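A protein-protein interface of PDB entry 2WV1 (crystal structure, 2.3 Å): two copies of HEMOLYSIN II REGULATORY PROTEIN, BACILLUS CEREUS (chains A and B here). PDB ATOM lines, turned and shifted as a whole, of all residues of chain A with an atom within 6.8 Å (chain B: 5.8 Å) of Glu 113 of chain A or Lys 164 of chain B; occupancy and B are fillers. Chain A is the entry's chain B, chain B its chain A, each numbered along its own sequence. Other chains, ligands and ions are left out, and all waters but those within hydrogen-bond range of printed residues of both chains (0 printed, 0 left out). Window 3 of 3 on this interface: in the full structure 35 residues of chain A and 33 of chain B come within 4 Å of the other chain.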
ATOM      1  N   GLU A 108      14.881  15.944  26.956  1.00  0.00           N
ATOM      2  CA  GLU A 108      16.154  15.344  27.393  1.00  0.00           C
ATOM      3  C   GLU A 108      17.332  16.100  26.808  1.00  0.00           C
ATOM      4  O   GLU A 108      17.964  16.841  27.538  1.00  0.00           O
ATOM      5  CB  GLU A 108      16.246  13.843  27.068  1.00  0.00           C
ATOM      6  CG  GLU A 108      17.644  13.211  27.333  1.00  0.00           C
ATOM      7  CD  GLU A 108      17.700  11.696  27.110  1.00  0.00           C
ATOM      8  OE1 GLU A 108      16.633  11.040  27.005  1.00  0.00           O
ATOM      9  OE2 GLU A 108      18.832  11.149  27.044  1.00  0.00           O
ATOM     10  N   GLU A 109      17.601  15.917  25.504  1.00  0.00           N
ATOM     11  CA  GLU A 109      18.674  16.595  24.734  1.00  0.00           C
ATOM     12  C   GLU A 109      18.889  18.084  25.025  1.00  0.00           C
ATOM     13  O   GLU A 109      19.970  18.608  24.779  1.00  0.00           O
ATOM     14  CB  GLU A 109      18.390  16.504  23.232  1.00  0.00           C
ATOM     15  CG  GLU A 109      18.193  15.125  22.676  1.00  0.00           C
ATOM     16  CD  GLU A 109      19.471  14.352  22.582  1.00  0.00           C
ATOM     17  OE1 GLU A 109      20.547  14.956  22.371  1.00  0.00           O
ATOM     18  OE2 GLU A 109      19.393  13.127  22.724  1.00  0.00           O
ATOM     19  N   ILE A 110      17.842  18.773  25.463  1.00  0.00           N
ATOM     20  CA  ILE A 110      17.967  20.143  25.956  1.00  0.00           C
ATOM     21  C   ILE A 110      18.892  20.213  27.189  1.00  0.00           C
ATOM     22  O   ILE A 110      19.620  21.181  27.359  1.00  0.00           O
ATOM     23  CB  ILE A 110      16.586  20.748  26.245  1.00  0.00           C
ATOM     24  CG1 ILE A 110      15.856  21.017  24.929  1.00  0.00           C
ATOM     25  CG2 ILE A 110      16.701  22.023  27.060  1.00  0.00           C
ATOM     26  CD1 ILE A 110      14.379  21.201  25.055  1.00  0.00           C
ATOM     27  N   ILE A 111      18.881  19.167  28.012  1.00  0.00           N
ATOM     28  CA  ILE A 111      19.794  19.026  29.152  1.00  0.00           C
ATOM     29  C   ILE A 111      21.238  18.621  28.771  1.00  0.00           C
ATOM     30  O   ILE A 111      22.199  19.149  29.331  1.00  0.00           O
ATOM     31  CB  ILE A 111      19.214  18.048  30.186  1.00  0.00           C
ATOM     32  CG1 ILE A 111      18.031  18.693  30.931  1.00  0.00           C
ATOM     33  CG2 ILE A 111      20.294  17.571  31.150  1.00  0.00           C
ATOM     34  CD1 ILE A 111      16.916  17.706  31.352  1.00  0.00           C
ATOM     35  N   LYS A 112      21.407  17.690  27.838  1.00  0.00           N
ATOM     36  CA  LYS A 112      22.763  17.328  27.394  1.00  0.00           C
ATOM     37  C   LYS A 112      23.420  18.395  26.500  1.00  0.00           C
ATOM     38  O   LYS A 112      24.636  18.369  26.275  1.00  0.00           O
ATOM     39  CB  LYS A 112      22.796  15.937  26.722  1.00  0.00           C
ATOM     40  CG  LYS A 112      23.302  14.798  27.630  1.00  0.00           C
ATOM     41  CD  LYS A 112      22.809  13.418  27.169  1.00  0.00           C
ATOM     42  CE  LYS A 112      23.047  12.351  28.243  1.00  0.00           C
ATOM     43  NZ  LYS A 112      22.596  10.992  27.809  1.00  0.00           N
ATOM     44  N   GLU A 113      22.607  19.320  25.993  1.00  0.00           N
ATOM     45  CA  GLU A 113      23.086  20.456  25.202  1.00  0.00           C
ATOM     46  C   GLU A 113      23.959  19.995  24.034  1.00  0.00           C
ATOM     47  O   GLU A 113      24.959  20.637  23.693  1.00  0.00           O
ATOM     48  CB  GLU A 113      23.816  21.469  26.112  1.00  0.00           C
ATOM     49  CG  GLU A 113      22.963  21.957  27.303  1.00  0.00           C
ATOM     50  CD  GLU A 113      23.679  22.932  28.237  1.00  0.00           C
ATOM     51  OE1 GLU A 113      24.707  22.553  28.840  1.00  0.00           O
ATOM     52  OE2 GLU A 113      23.192  24.076  28.393  1.00  0.00           O
ATOM     53  N   SER A 114      23.559  18.872  23.428  1.00  0.00           N
ATOM     54  CA  SER A 114      24.377  18.142  22.457  1.00  0.00           C
ATOM     55  C   SER A 114      24.290  18.724  21.047  1.00  0.00           C
ATOM     56  O   SER A 114      23.422  19.557  20.759  1.00  0.00           O
ATOM     57  CB  SER A 114      23.997  16.661  22.453  1.00  0.00           C
ATOM     58  OG  SER A 114      22.601  16.488  22.652  1.00  0.00           O
ATOM     59  N   ALA A 115      25.206  18.296  20.177  1.00  0.00           N
ATOM     60  CA  ALA A 115      25.198  18.719  18.773  1.00  0.00           C
ATOM     61  C   ALA A 115      23.925  18.214  18.089  1.00  0.00           C
ATOM     62  O   ALA A 115      23.427  18.821  17.127  1.00  0.00           O
ATOM     63  CB  ALA A 115      26.432  18.212  18.056  1.00  0.00           C
ATOM     64  N   ARG A 116      23.404  17.102  18.612  1.00  0.00           N
ATOM     65  CA  ARG A 116      22.115  16.578  18.194  1.00  0.00           C
ATOM     66  C   ARG A 116      21.015  17.612  18.421  1.00  0.00           C
ATOM     67  O   ARG A 116      20.160  17.799  17.549  1.00  0.00           O
ATOM     68  CB  ARG A 116      21.785  15.275  18.924  1.00  0.00           C
ATOM     69  CG  ARG A 116      22.669  14.118  18.504  1.00  0.00           C
ATOM     70  CD  ARG A 116      22.069  12.788  18.878  1.00  0.00           C
ATOM     71  NE  ARG A 116      21.648  12.756  20.270  1.00  0.00           N
ATOM     72  CZ  ARG A 116      22.456  12.489  21.291  1.00  0.00           C
ATOM     73  NH1 ARG A 116      23.747  12.216  21.079  1.00  0.00           N
ATOM     74  NH2 ARG A 116      21.966  12.490  22.529  1.00  0.00           N
ATOM     75  N   LEU A 117      21.055  18.305  19.563  1.00  0.00           N
ATOM     76  CA  LEU A 117      20.048  19.319  19.862  1.00  0.00           C
ATOM     77  C   LEU A 117      19.831  20.258  18.678  1.00  0.00           C
ATOM     78  O   LEU A 117      18.680  20.523  18.312  1.00  0.00           O
ATOM     79  CB  LEU A 117      20.367  20.100  21.151  1.00  0.00           C
ATOM     80  CG  LEU A 117      19.378  21.189  21.590  1.00  0.00           C
ATOM     81  CD1 LEU A 117      17.954  20.677  21.628  1.00  0.00           C
ATOM     82  CD2 LEU A 117      19.752  21.768  22.954  1.00  0.00           C
ATOM     83  N   GLU A 118      20.926  20.723  18.073  1.00  0.00           N
ATOM     84  CA  GLU A 118      20.849  21.704  16.983  1.00  0.00           C
ATOM     85  C   GLU A 118      20.084  21.164  15.789  1.00  0.00           C
ATOM     86  O   GLU A 118      19.201  21.837  15.276  1.00  0.00           O
ATOM     87  CB  GLU A 118      22.233  22.237  16.561  1.00  0.00           C
ATOM     88  CG  GLU A 118      23.001  22.997  17.660  1.00  0.00           C
ATOM     89  CD  GLU A 118      22.122  23.969  18.481  1.00  0.00           C
ATOM     90  OE1 GLU A 118      21.386  24.797  17.883  1.00  0.00           O
ATOM     91  OE2 GLU A 118      22.173  23.902  19.734  1.00  0.00           O
ATOM     92  N   THR B 104      18.163  16.790  36.753  1.00  0.00           N
ATOM     93  CA  THR B 104      18.012  16.093  35.487  1.00  0.00           C
ATOM     94  C   THR B 104      17.532  14.676  35.696  1.00  0.00           C
ATOM     95  O   THR B 104      16.856  14.107  34.829  1.00  0.00           O
ATOM     96  CB  THR B 104      19.306  16.151  34.649  1.00  0.00           C
ATOM     97  OG1 THR B 104      20.243  15.131  35.072  1.00  0.00           O
ATOM     98  CG2 THR B 104      19.933  17.549  34.794  1.00  0.00           C
ATOM     99  N   ILE B 159      11.230  25.989  36.500  1.00  0.00           N
ATOM    100  CA  ILE B 159      12.474  26.766  36.379  1.00  0.00           C
ATOM    101  C   ILE B 159      13.529  26.202  37.309  1.00  0.00           C
ATOM    102  O   ILE B 159      14.669  26.053  36.928  1.00  0.00           O
ATOM    103  CB  ILE B 159      12.249  28.234  36.754  1.00  0.00           C
ATOM    104  CG1 ILE B 159      11.384  28.910  35.680  1.00  0.00           C
ATOM    105  CG2 ILE B 159      13.608  28.977  36.988  1.00  0.00           C
ATOM    106  CD1 ILE B 159      10.759  30.226  36.105  1.00  0.00           C
ATOM    107  N   PHE B 162      14.467  22.416  36.317  1.00  0.00           N
ATOM    108  CA  PHE B 162      14.869  22.305  34.919  1.00  0.00           C
ATOM    109  C   PHE B 162      15.342  23.661  34.401  1.00  0.00           C
ATOM    110  O   PHE B 162      14.857  24.165  33.370  1.00  0.00           O
ATOM    111  CB  PHE B 162      13.718  21.731  34.076  1.00  0.00           C
ATOM    112  CG  PHE B 162      13.160  20.446  34.621  1.00  0.00           C
ATOM    113  CD1 PHE B 162      13.912  19.282  34.585  1.00  0.00           C
ATOM    114  CD2 PHE B 162      11.896  20.402  35.183  1.00  0.00           C
ATOM    115  CE1 PHE B 162      13.420  18.088  35.094  1.00  0.00           C
ATOM    116  CE2 PHE B 162      11.382  19.203  35.696  1.00  0.00           C
ATOM    117  CZ  PHE B 162      12.146  18.056  35.651  1.00  0.00           C
ATOM    118  N   PRO B 163      16.330  24.264  35.107  1.00  0.00           N
ATOM    119  CA  PRO B 163      16.858  25.567  34.677  1.00  0.00           C
ATOM    120  C   PRO B 163      17.295  25.566  33.233  1.00  0.00           C
ATOM    121  O   PRO B 163      17.272  26.591  32.618  1.00  0.00           O
ATOM    122  CB  PRO B 163      18.111  25.773  35.564  1.00  0.00           C
ATOM    123  CG  PRO B 163      18.533  24.338  35.932  1.00  0.00           C
ATOM    124  CD  PRO B 163      17.195  23.643  36.134  1.00  0.00           C
ATOM    125  N   LYS B 164      17.734  24.437  32.696  1.00  0.00           N
ATOM    126  CA  LYS B 164      18.259  24.444  31.318  1.00  0.00           C
ATOM    127  C   LYS B 164      17.207  24.702  30.224  1.00  0.00           C
ATOM    128  O   LYS B 164      17.545  25.223  29.168  1.00  0.00           O
ATOM    129  CB  LYS B 164      19.069  23.181  31.019  1.00  0.00           C
ATOM    130  CG  LYS B 164      20.489  23.235  31.571  1.00  0.00           C
ATOM    131  CD  LYS B 164      21.326  22.044  31.068  1.00  0.00           C
ATOM    132  CE  LYS B 164      22.528  21.766  31.957  1.00  0.00           C
ATOM    133  NZ  LYS B 164      23.672  22.628  31.581  1.00  0.00           N
ATOM    134  N   PHE B 165      15.955  24.330  30.483  1.00  0.00           N
ATOM    135  CA  PHE B 165      14.861  24.593  29.547  1.00  0.00           C
ATOM    136  C   PHE B 165      14.533  26.064  29.585  1.00  0.00           C
ATOM    137  O   PHE B 165      14.259  26.665  28.561  1.00  0.00           O
ATOM    138  CB  PHE B 165      13.604  23.789  29.899  1.00  0.00           C
ATOM    139  CG  PHE B 165      12.504  23.896  28.880  1.00  0.00           C
ATOM    140  CD1 PHE B 165      12.640  23.320  27.617  1.00  0.00           C
ATOM    141  CD2 PHE B 165      11.332  24.576  29.182  1.00  0.00           C
ATOM    142  CE1 PHE B 165      11.624  23.414  26.678  1.00  0.00           C
ATOM    143  CE2 PHE B 165      10.310  24.665  28.253  1.00  0.00           C
ATOM    144  CZ  PHE B 165      10.456  24.088  26.996  1.00  0.00           C
ATOM    145  N   LYS B 166      14.581  26.633  30.783  1.00  0.00           N
ATOM    146  CA  LYS B 166      14.398  28.060  30.965  1.00  0.00           C
ATOM    147  C   LYS B 166      15.430  28.837  30.143  1.00  0.00           C
ATOM    148  O   LYS B 166      15.071  29.753  29.402  1.00  0.00           O
ATOM    149  CB  LYS B 166      14.442  28.436  32.452  1.00  0.00           C
ATOM    150  CG  LYS B 166      14.302  29.935  32.703  1.00  0.00           C
ATOM    151  CD  LYS B 166      12.895  30.445  32.325  1.00  0.00           C
ATOM    152  CE  LYS B 166      12.748  31.951  32.577  1.00  0.00           C
ATOM    153  NZ  LYS B 166      11.378  32.448  32.264  1.00  0.00           N
ATOM    154  N   LYS B 167      16.694  28.449  30.236  1.00  0.00           N
ATOM    155  CA  LYS B 167      17.725  29.055  29.383  1.00  0.00           C
ATOM    156  C   LYS B 167      17.482  28.839  27.888  1.00  0.00           C
ATOM    157  O   LYS B 167      17.748  29.727  27.085  1.00  0.00           O
ATOM    158  CB  LYS B 167      19.132  28.566  29.771  1.00  0.00           C
ATOM    159  CG  LYS B 167      19.620  29.134  31.112  1.00  0.00           C
ATOM    160  CD  LYS B 167      21.148  29.125  31.216  1.00  0.00           C
ATOM    161  CE  LYS B 167      21.610  29.937  32.426  1.00  0.00           C
ATOM    162  NZ  LYS B 167      23.011  30.418  32.221  1.00  0.00           N
ATOM    163  N   PHE B 168      16.978  27.660  27.526  1.00  0.00           N
ATOM    164  CA  PHE B 168      16.723  27.298  26.127  1.00  0.00           C
ATOM    165  C   PHE B 168      15.673  28.226  25.532  1.00  0.00           C
ATOM    166  O   PHE B 168      15.847  28.732  24.432  1.00  0.00           O
ATOM    167  CB  PHE B 168      16.239  25.851  26.071  1.00  0.00           C
ATOM    168  CG  PHE B 168      15.901  25.351  24.688  1.00  0.00           C
ATOM    169  CD1 PHE B 168      14.561  25.166  24.305  1.00  0.00           C
ATOM    170  CD2 PHE B 168      16.908  25.031  23.780  1.00  0.00           C
ATOM    171  CE1 PHE B 168      14.236  24.675  23.017  1.00  0.00           C
ATOM    172  CE2 PHE B 168      16.594  24.530  22.494  1.00  0.00           C
ATOM    173  CZ  PHE B 168      15.256  24.357  22.117  1.00  0.00           C
ATOM    174  N   ILE B 169      14.592  28.443  26.275  1.00  0.00           N
ATOM    175  CA  ILE B 169      13.530  29.384  25.885  1.00  0.00           C
ATOM    176  C   ILE B 169      14.044  30.834  25.878  1.00  0.00           C
ATOM    177  O   ILE B 169      13.727  31.598  24.963  1.00  0.00           O
ATOM    178  CB  ILE B 169      12.276  29.267  26.809  1.00  0.00           C
ATOM    179  CG1 ILE B 169      11.657  27.866  26.704  1.00  0.00           C
ATOM    180  CG2 ILE B 169      11.238  30.380  26.496  1.00  0.00           C
ATOM    181  CD1 ILE B 169      11.156  27.492  25.304  1.00  0.00           C
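The side-chain amino group (NZ) of Lys 164 of chain B lies within salt-bridge range of the side-chain carboxylate (OE1) of Glu 113 of chain A (2.9 Å).
Ile 110 of chain A touches Lys 164 of chain B (CG2 to O, 3.9 Å). Ile 110 of chain A touches Phe 165 of chain B. Phe 168 of chain B touches Ile 110 of chain A. Thr 104 of chain B touches Ile 111 of chain A (CG2 to CG2, 3.7 Å). Lys 164 of chain B touches Ile 111 of chain A (CD to O, 3.5 Å).
Printed residues of chain B within 4 Å of Ile 110 of chain A: Lys 164, Phe 165 and Phe 168. Of the printed residues of chain B, Ile 111 of chain A touches Thr 104 and Lys 164. Glu 113 of chain A touches just one residue of chain B: Lys 164 (2.9 Å). Of the printed residues of chain A, Thr 104 of chain B touches Ile 111 (3.7 Å). Of chain A, only Ile 110 (3.9 Å), Ile 111 (3.5 Å) and Glu 113 (2.9 Å) come within 4 Å of Lys 164 of chain B. Of the printed residues of chain A, Phe 165 of chain B touches Ile 110. Of the printed residues of chain A, Phe 168 of chain B touches Ile 110 (3.98 Å). The nearest printed residue of chain B that does not touch Glu 113 of chain A is Lys 167 of chain B (6.1 Å).
Of the 11 printed residues of chain A, 3 touch a printed residue of chain B. Hydrophobic or aromatic side chains of chain A that line the printed part of chain B: Ile 110 and Ile 111. Hydrophobic or aromatic side chains of chain B that line the printed part of chain A: Phe 165 and Phe 168. Among the printed residues, 6 pairs touch across the chains. Among the printed residues, Asp or Glu carboxylates within 4 Å of a Lys or Arg side-chain nitrogen of the other chain: Glu 113 of chain A with Lys 164 of chain B (2.9 Å).
No position is printed for both chains.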
